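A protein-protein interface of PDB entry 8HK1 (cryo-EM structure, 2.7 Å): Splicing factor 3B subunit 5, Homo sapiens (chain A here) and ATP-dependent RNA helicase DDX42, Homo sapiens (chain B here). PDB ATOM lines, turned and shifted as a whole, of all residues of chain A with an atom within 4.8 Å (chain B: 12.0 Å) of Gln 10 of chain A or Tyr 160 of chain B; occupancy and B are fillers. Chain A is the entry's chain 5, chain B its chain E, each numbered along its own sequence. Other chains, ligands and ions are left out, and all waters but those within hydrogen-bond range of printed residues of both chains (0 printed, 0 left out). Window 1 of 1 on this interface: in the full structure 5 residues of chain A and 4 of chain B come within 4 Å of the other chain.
The side-chain hydroxyl (OH) of Tyr 160 of chain B lies within hydrogen-bond range of the side-chain hydroxyl (OG) of Ser 9 of chain A (2.6 Å).
The side-chain hydroxyl (OG) of Ser 9 of chain A sits at hydrogen-bond distance from the backbone carbonyl oxygen (O) of Thr 6 of chain A (2.5 Å).
O of Thr 6 of chain A touches OH of Tyr 160 of chain B (3.5 Å). CA of Gln 10 of chain A touches CE2 of Tyr 160 of chain B (3.8 Å). O of Ala 159 of chain B touches NE2 of His 13 of chain A, 3.8 Å away. His 13 of chain A touches Tyr 160 of chain B. Tyr 163 of chain B touches His 13 of chain A.
Gln 10 of chain A touches one residue of chain B. Tyr 160 of chain B touches four residues of chain A. Of chain B, only Tyr 160 comes within 4 Å of Thr 6 of chain A. Glu 12 of chain A touches none of the printed residues of chain B. His 13 of chain A touches just these residues of chain B: Ala 159, Tyr 160 and Tyr 163. Of the printed residues of chain A, Tyr 163 of chain B touches His 13. Of the printed residues of chain A, Ala 159 of chain B touches His 13 (3.8 Å). Asp 155 of chain B touches none of the printed residues of chain A. Met 164 of chain B touches none of the printed residues of chain A. The nearest residue of chain B that does not touch Gln 10 of chain A is Met 164 of chain B (6.4 Å). The nearest printed residue of chain A that does not touch Tyr 160 of chain B is Ile 7 of chain A (5.6 Å).
Hydrophobic or aromatic side chains of chain B within 4 Å of the printed part of chain A: Tyr 160 and Tyr 163. Hydrophobic or aromatic side chains of chain A within 4 Å of the printed part of chain B: His 13. Among the printed residues, no Asp or Glu carboxylate lies within 4 Å of a Lys or Arg side-chain nitrogen of the other chain.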
ATOM      1  N   THR A   6      14.751  35.893  17.173  1.00  0.00           N
ATOM      2  CA  THR A   6      14.359  34.572  16.611  1.00  0.00           C
ATOM      3  C   THR A   6      13.738  33.704  17.709  1.00  0.00           C
ATOM      4  O   THR A   6      13.323  32.576  17.390  1.00  0.00           O
ATOM      5  CB  THR A   6      15.558  33.853  15.979  1.00  0.00           C
ATOM      6  OG1 THR A   6      16.657  33.943  16.887  1.00  0.00           O
ATOM      7  CG2 THR A   6      15.956  34.424  14.636  1.00  0.00           C
ATOM      8  N   ILE A   7      13.639  34.230  18.934  1.00  0.00           N
ATOM      9  CA  ILE A   7      13.078  33.466  20.090  1.00  0.00           C
ATOM     10  C   ILE A   7      11.622  33.095  19.780  1.00  0.00           C
ATOM     11  O   ILE A   7      11.232  31.942  20.059  1.00  0.00           O
ATOM     12  CB  ILE A   7      13.171  34.300  21.384  1.00  0.00           C
ATOM     13  CG1 ILE A   7      13.953  35.599  21.176  1.00  0.00           C
ATOM     14  CG2 ILE A   7      13.723  33.471  22.533  1.00  0.00           C
ATOM     15  CD1 ILE A   7      14.473  36.213  22.456  1.00  0.00           C
ATOM     16  N   HIS A   8      10.871  34.035  19.199  1.00  0.00           N
ATOM     17  CA  HIS A   8       9.443  33.808  18.848  1.00  0.00           C
ATOM     18  C   HIS A   8       9.350  32.677  17.822  1.00  0.00           C
ATOM     19  O   HIS A   8       8.468  31.819  17.973  1.00  0.00           O
ATOM     20  CB  HIS A   8       8.834  35.111  18.318  1.00  0.00           C
ATOM     21  CG  HIS A   8       9.679  36.309  18.598  1.00  0.00           C
ATOM     22  ND1 HIS A   8      10.241  36.540  19.838  1.00  0.00           N
ATOM     23  CD2 HIS A   8      10.066  37.335  17.809  1.00  0.00           C
ATOM     24  CE1 HIS A   8      10.936  37.659  19.801  1.00  0.00           C
ATOM     25  NE2 HIS A   8      10.843  38.167  18.568  1.00  0.00           N
ATOM     26  N   SER A   9      10.246  32.682  16.831  1.00  0.00           N
ATOM     27  CA  SER A   9      10.301  31.635  15.777  1.00  0.00           C
ATOM     28  C   SER A   9      10.621  30.280  16.418  1.00  0.00           C
ATOM     29  O   SER A   9      10.013  29.278  16.005  1.00  0.00           O
ATOM     30  CB  SER A   9      11.314  31.989  14.722  1.00  0.00           C
ATOM     31  OG  SER A   9      12.622  31.632  15.140  1.00  0.00           O
ATOM     32  N   GLN A  10      11.542  30.256  17.390  1.00  0.00           N
ATOM     33  CA  GLN A  10      11.884  28.987  18.090  1.00  0.00           C
ATOM     34  C   GLN A  10      10.646  28.485  18.831  1.00  0.00           C
ATOM     35  O   GLN A  10      10.378  27.271  18.787  1.00  0.00           O
ATOM     36  CB  GLN A  10      12.961  29.208  19.147  1.00  0.00           C
ATOM     37  CG  GLN A  10      13.386  27.921  19.836  1.00  0.00           C
ATOM     38  CD  GLN A  10      13.916  28.163  21.226  1.00  0.00           C
ATOM     39  OE1 GLN A  10      13.763  29.242  21.792  1.00  0.00           O
ATOM     40  NE2 GLN A  10      14.579  27.159  21.776  1.00  0.00           N
ATOM     41  N   LEU A  11       9.909  29.404  19.464  1.00  0.00           N
ATOM     42  CA  LEU A  11       8.671  29.036  20.199  1.00  0.00           C
ATOM     43  C   LEU A  11       7.679  28.443  19.192  1.00  0.00           C
ATOM     44  O   LEU A  11       7.073  27.401  19.503  1.00  0.00           O
ATOM     45  CB  LEU A  11       8.112  30.305  20.851  1.00  0.00           C
ATOM     46  CG  LEU A  11       6.976  30.095  21.849  1.00  0.00           C
ATOM     47  CD1 LEU A  11       5.715  29.619  21.146  1.00  0.00           C
ATOM     48  CD2 LEU A  11       7.383  29.120  22.941  1.00  0.00           C
ATOM     49  N   GLU A  12       7.566  29.062  18.012  1.00  0.00           N
ATOM     50  CA  GLU A  12       6.673  28.570  16.933  1.00  0.00           C
ATOM     51  C   GLU A  12       7.157  27.197  16.454  1.00  0.00           C
ATOM     52  O   GLU A  12       6.323  26.449  15.906  1.00  0.00           O
ATOM     53  CB  GLU A  12       6.630  29.556  15.763  1.00  0.00           C
ATOM     54  CG  GLU A  12       6.010  30.895  16.116  1.00  0.00           C
ATOM     55  CD  GLU A  12       6.159  31.963  15.046  1.00  0.00           C
ATOM     56  OE1 GLU A  12       5.728  31.719  13.902  1.00  0.00           O
ATOM     57  OE2 GLU A  12       6.713  33.035  15.357  1.00  0.00           O
ATOM     58  N   HIS A  13       8.451  26.886  16.609  1.00  0.00           N
ATOM     59  CA  HIS A  13       8.917  25.546  16.159  1.00  0.00           C
ATOM     60  C   HIS A  13       8.726  24.501  17.270  1.00  0.00           C
ATOM     61  O   HIS A  13       8.485  23.328  16.934  1.00  0.00           O
ATOM     62  CB  HIS A  13      10.382  25.640  15.706  1.00  0.00           C
ATOM     63  CG  HIS A  13      10.884  24.426  15.001  1.00  0.00           C
ATOM     64  ND1 HIS A  13      11.498  23.387  15.671  1.00  0.00           N
ATOM     65  CD2 HIS A  13      10.877  24.084  13.694  1.00  0.00           C
ATOM     66  CE1 HIS A  13      11.842  22.453  14.809  1.00  0.00           C
ATOM     67  NE2 HIS A  13      11.473  22.857  13.589  1.00  0.00           N
ATOM     68  N   LEU A  14       8.834  24.919  18.536  1.00  0.00           N
ATOM     69  CA  LEU A  14       8.705  24.031  19.721  1.00  0.00           C
ATOM     70  C   LEU A  14       7.226  23.700  19.943  1.00  0.00           C
ATOM     71  O   LEU A  14       6.928  22.554  20.318  1.00  0.00           O
ATOM     72  CB  LEU A  14       9.319  24.732  20.936  1.00  0.00           C
ATOM     73  CG  LEU A  14      10.845  24.813  20.935  1.00  0.00           C
ATOM     74  CD1 LEU A  14      11.352  25.574  22.150  1.00  0.00           C
ATOM     75  CD2 LEU A  14      11.466  23.428  20.878  1.00  0.00           C
ATOM     76  N   GLU B 153      19.420   9.951  14.362  1.00  0.00           N
ATOM     77  CA  GLU B 153      18.222  10.830  14.245  1.00  0.00           C
ATOM     78  C   GLU B 153      18.562  12.298  14.535  1.00  0.00           C
ATOM     79  O   GLU B 153      19.171  12.574  15.578  1.00  0.00           O
ATOM     80  CB  GLU B 153      17.099  10.317  15.149  1.00  0.00           C
ATOM     81  CG  GLU B 153      16.548   8.971  14.713  1.00  0.00           C
ATOM     82  CD  GLU B 153      15.750   8.234  15.775  1.00  0.00           C
ATOM     83  OE1 GLU B 153      15.619   8.772  16.890  1.00  0.00           O
ATOM     84  OE2 GLU B 153      15.265   7.122  15.483  1.00  0.00           O
ATOM     85  N   GLU B 154      18.108  13.207  13.667  1.00  0.00           N
ATOM     86  CA  GLU B 154      18.366  14.662  13.835  1.00  0.00           C
ATOM     87  C   GLU B 154      17.877  15.134  15.207  1.00  0.00           C
ATOM     88  O   GLU B 154      16.772  14.738  15.616  1.00  0.00           O
ATOM     89  CB  GLU B 154      17.616  15.449  12.757  1.00  0.00           C
ATOM     90  CG  GLU B 154      18.382  15.590  11.458  1.00  0.00           C
ATOM     91  CD  GLU B 154      17.719  16.509  10.447  1.00  0.00           C
ATOM     92  OE1 GLU B 154      16.560  16.904  10.682  1.00  0.00           O
ATOM     93  OE2 GLU B 154      18.362  16.829   9.428  1.00  0.00           O
ATOM     94  N   ASP B 155      18.630  16.057  15.821  1.00  0.00           N
ATOM     95  CA  ASP B 155      18.280  16.646  17.142  1.00  0.00           C
ATOM     96  C   ASP B 155      17.266  17.781  16.936  1.00  0.00           C
ATOM     97  O   ASP B 155      17.060  18.191  15.777  1.00  0.00           O
ATOM     98  CB  ASP B 155      19.518  17.190  17.856  1.00  0.00           C
ATOM     99  CG  ASP B 155      20.830  16.655  17.307  1.00  0.00           C
ATOM    100  OD1 ASP B 155      20.784  15.756  16.445  1.00  0.00           O
ATOM    101  OD2 ASP B 155      21.888  17.151  17.743  1.00  0.00           O
ATOM    102  N   ASP B 156      16.682  18.288  18.025  1.00  0.00           N
ATOM    103  CA  ASP B 156      15.674  19.377  17.929  1.00  0.00           C
ATOM    104  C   ASP B 156      16.328  20.620  17.320  1.00  0.00           C
ATOM    105  O   ASP B 156      15.706  21.242  16.436  1.00  0.00           O
ATOM    106  CB  ASP B 156      15.106  19.716  19.309  1.00  0.00           C
ATOM    107  CG  ASP B 156      15.192  18.565  20.293  1.00  0.00           C
ATOM    108  OD1 ASP B 156      15.487  17.436  19.850  1.00  0.00           O
ATOM    109  OD2 ASP B 156      14.963  18.807  21.496  1.00  0.00           O
ATOM    110  N   GLN B 157      17.551  20.941  17.752  1.00  0.00           N
ATOM    111  CA  GLN B 157      18.279  22.126  17.227  1.00  0.00           C
ATOM    112  C   GLN B 157      18.540  21.934  15.729  1.00  0.00           C
ATOM    113  O   GLN B 157      18.334  22.900  14.968  1.00  0.00           O
ATOM    114  CB  GLN B 157      19.584  22.333  17.995  1.00  0.00           C
ATOM    115  CG  GLN B 157      19.400  23.033  19.333  1.00  0.00           C
ATOM    116  CD  GLN B 157      20.712  23.513  19.902  1.00  0.00           C
ATOM    117  OE1 GLN B 157      21.753  23.442  19.253  1.00  0.00           O
ATOM    118  NE2 GLN B 157      20.671  24.009  21.128  1.00  0.00           N
ATOM    119  N   GLU B 158      18.938  20.724  15.321  1.00  0.00           N
ATOM    120  CA  GLU B 158      19.207  20.447  13.885  1.00  0.00           C
ATOM    121  C   GLU B 158      17.908  20.632  13.096  1.00  0.00           C
ATOM    122  O   GLU B 158      17.954  21.250  12.018  1.00  0.00           O
ATOM    123  CB  GLU B 158      19.748  19.027  13.701  1.00  0.00           C
ATOM    124  CG  GLU B 158      21.250  18.925  13.891  1.00  0.00           C
ATOM    125  CD  GLU B 158      21.864  17.619  13.417  1.00  0.00           C
ATOM    126  OE1 GLU B 158      21.117  16.768  12.897  1.00  0.00           O
ATOM    127  OE2 GLU B 158      23.091  17.456  13.569  1.00  0.00           O
ATOM    128  N   ALA B 159      16.788  20.151  13.647  1.00  0.00           N
ATOM    129  CA  ALA B 159      15.477  20.275  12.973  1.00  0.00           C
ATOM    130  C   ALA B 159      15.135  21.760  12.816  1.00  0.00           C
ATOM    131  O   ALA B 159      14.696  22.151  11.721  1.00  0.00           O
ATOM    132  CB  ALA B 159      14.428  19.554  13.783  1.00  0.00           C
ATOM    133  N   TYR B 160      15.383  22.556  13.859  1.00  0.00           N
ATOM    134  CA  TYR B 160      15.094  24.013  13.810  1.00  0.00           C
ATOM    135  C   TYR B 160      15.955  24.671  12.727  1.00  0.00           C
ATOM    136  O   TYR B 160      15.426  25.497  11.958  1.00  0.00           O
ATOM    137  CB  TYR B 160      15.358  24.658  15.172  1.00  0.00           C
ATOM    138  CG  TYR B 160      15.234  26.160  15.182  1.00  0.00           C
ATOM    139  CD1 TYR B 160      16.338  26.966  15.395  1.00  0.00           C
ATOM    140  CD2 TYR B 160      14.015  26.779  14.964  1.00  0.00           C
ATOM    141  CE1 TYR B 160      16.236  28.346  15.401  1.00  0.00           C
ATOM    142  CE2 TYR B 160      13.895  28.158  14.967  1.00  0.00           C
ATOM    143  CZ  TYR B 160      15.009  28.947  15.186  1.00  0.00           C
ATOM    144  OH  TYR B 160      14.899  30.307  15.188  1.00  0.00           O
ATOM    145  N   PHE B 161      17.234  24.289  12.648  1.00  0.00           N
ATOM    146  CA  PHE B 161      18.143  24.876  11.628  1.00  0.00           C
ATOM    147  C   PHE B 161      17.624  24.513  10.232  1.00  0.00           C
ATOM    148  O   PHE B 161      17.577  25.397   9.350  1.00  0.00           O
ATOM    149  CB  PHE B 161      19.576  24.384  11.838  1.00  0.00           C
ATOM    150  CG  PHE B 161      20.216  24.832  13.129  1.00  0.00           C
ATOM    151  CD1 PHE B 161      19.938  26.077  13.665  1.00  0.00           C
ATOM    152  CD2 PHE B 161      21.114  24.014  13.796  1.00  0.00           C
ATOM    153  CE1 PHE B 161      20.528  26.489  14.849  1.00  0.00           C
ATOM    154  CE2 PHE B 161      21.705  24.427  14.981  1.00  0.00           C
ATOM    155  CZ  PHE B 161      21.412  25.663  15.504  1.00  0.00           C
ATOM    156  N   ARG B 162      17.186  23.263  10.068  1.00  0.00           N
ATOM    157  CA  ARG B 162      16.663  22.790   8.760  1.00  0.00           C
ATOM    158  C   ARG B 162      15.429  23.621   8.402  1.00  0.00           C
ATOM    159  O   ARG B 162      15.345  24.082   7.250  1.00  0.00           O
ATOM    160  CB  ARG B 162      16.277  21.312   8.871  1.00  0.00           C
ATOM    161  CG  ARG B 162      17.460  20.360   8.963  1.00  0.00           C
ATOM    162  CD  ARG B 162      17.569  19.465   7.745  1.00  0.00           C
ATOM    163  NE  ARG B 162      16.641  18.345   7.824  1.00  0.00           N
ATOM    164  CZ  ARG B 162      15.331  18.435   7.632  1.00  0.00           C
ATOM    165  NH1 ARG B 162      14.783  19.605   7.352  1.00  0.00           N
ATOM    166  NH2 ARG B 162      14.573  17.358   7.725  1.00  0.00           N
ATOM    167  N   TYR B 163      14.553  23.859   9.380  1.00  0.00           N
ATOM    168  CA  TYR B 163      13.311  24.641   9.142  1.00  0.00           C
ATOM    169  C   TYR B 163      13.677  26.066   8.721  1.00  0.00           C
ATOM    170  O   TYR B 163      13.091  26.568   7.743  1.00  0.00           O
ATOM    171  CB  TYR B 163      12.454  24.669  10.410  1.00  0.00           C
ATOM    172  CG  TYR B 163      11.115  25.342  10.243  1.00  0.00           C
ATOM    173  CD1 TYR B 163      10.928  26.663  10.612  1.00  0.00           C
ATOM    174  CD2 TYR B 163      10.034  24.658   9.712  1.00  0.00           C
ATOM    175  CE1 TYR B 163       9.701  27.289  10.460  1.00  0.00           C
ATOM    176  CE2 TYR B 163       8.802  25.269   9.554  1.00  0.00           C
ATOM    177  CZ  TYR B 163       8.634  26.589   9.928  1.00  0.00           C
ATOM    178  OH  TYR B 163       7.419  27.193   9.774  1.00  0.00           O
ATOM    179  N   MET B 164      14.656  26.675   9.398  1.00  0.00           N
ATOM    180  CA  MET B 164      15.054  28.063   9.044  1.00  0.00           C
ATOM    181  C   MET B 164      15.598  28.076   7.611  1.00  0.00           C
ATOM    182  O   MET B 164      15.191  28.963   6.835  1.00  0.00           O
ATOM    183  CB  MET B 164      16.124  28.594  10.003  1.00  0.00           C
ATOM    184  CG  MET B 164      15.621  28.778  11.421  1.00  0.00           C
ATOM    185  SD  MET B 164      13.991  29.568  11.489  1.00  0.00           S
ATOM    186  CE  MET B 164      14.388  31.211  10.893  1.00  0.00           C
ATOM    187  N   ALA B 165      16.420  27.082   7.257  1.00  0.00           N
ATOM    188  CA  ALA B 165      16.997  27.030   5.894  1.00  0.00           C
ATOM    189  C   ALA B 165      15.867  26.891   4.865  1.00  0.00           C
ATOM    190  O   ALA B 165      15.905  27.604   3.844  1.00  0.00           O
ATOM    191  CB  ALA B 165      17.969  25.881   5.800  1.00  0.00           C
ATOM    192  N   GLU B 166      14.880  26.038   5.155  1.00  0.00           N
ATOM    193  CA  GLU B 166      13.740  25.813   4.226  1.00  0.00           C
ATOM    194  C   GLU B 166      12.937  27.109   4.063  1.00  0.00           C
ATOM    195  O   GLU B 166      12.571  27.428   2.915  1.00  0.00           O
ATOM    196  CB  GLU B 166      12.873  24.653   4.720  1.00  0.00           C
ATOM    197  CG  GLU B 166      13.584  23.310   4.668  1.00  0.00           C
ATOM    198  CD  GLU B 166      12.687  22.092   4.822  1.00  0.00           C
ATOM    199  OE1 GLU B 166      11.524  22.155   4.377  1.00  0.00           O
ATOM    200  OE2 GLU B 166      13.155  21.083   5.385  1.00  0.00           O
ATOM    201  N   ASN B 167      12.714  27.846   5.155  1.00  0.00           N
ATOM    202  CA  ASN B 167      11.928  29.109   5.090  1.00  0.00           C
ATOM    203  C   ASN B 167      12.159  29.932   6.360  1.00  0.00           C
ATOM    204  O   ASN B 167      12.633  31.075   6.219  1.00  0.00           O
ATOM    205  CB  ASN B 167      10.437  28.832   4.875  1.00  0.00           C
ATOM    206  CG  ASN B 167       9.858  27.886   5.906  1.00  0.00           C
ATOM    207  OD1 ASN B 167       9.923  28.150   7.105  1.00  0.00           O
ATOM    208  ND2 ASN B 167       9.284  26.785   5.449  1.00  0.00           N
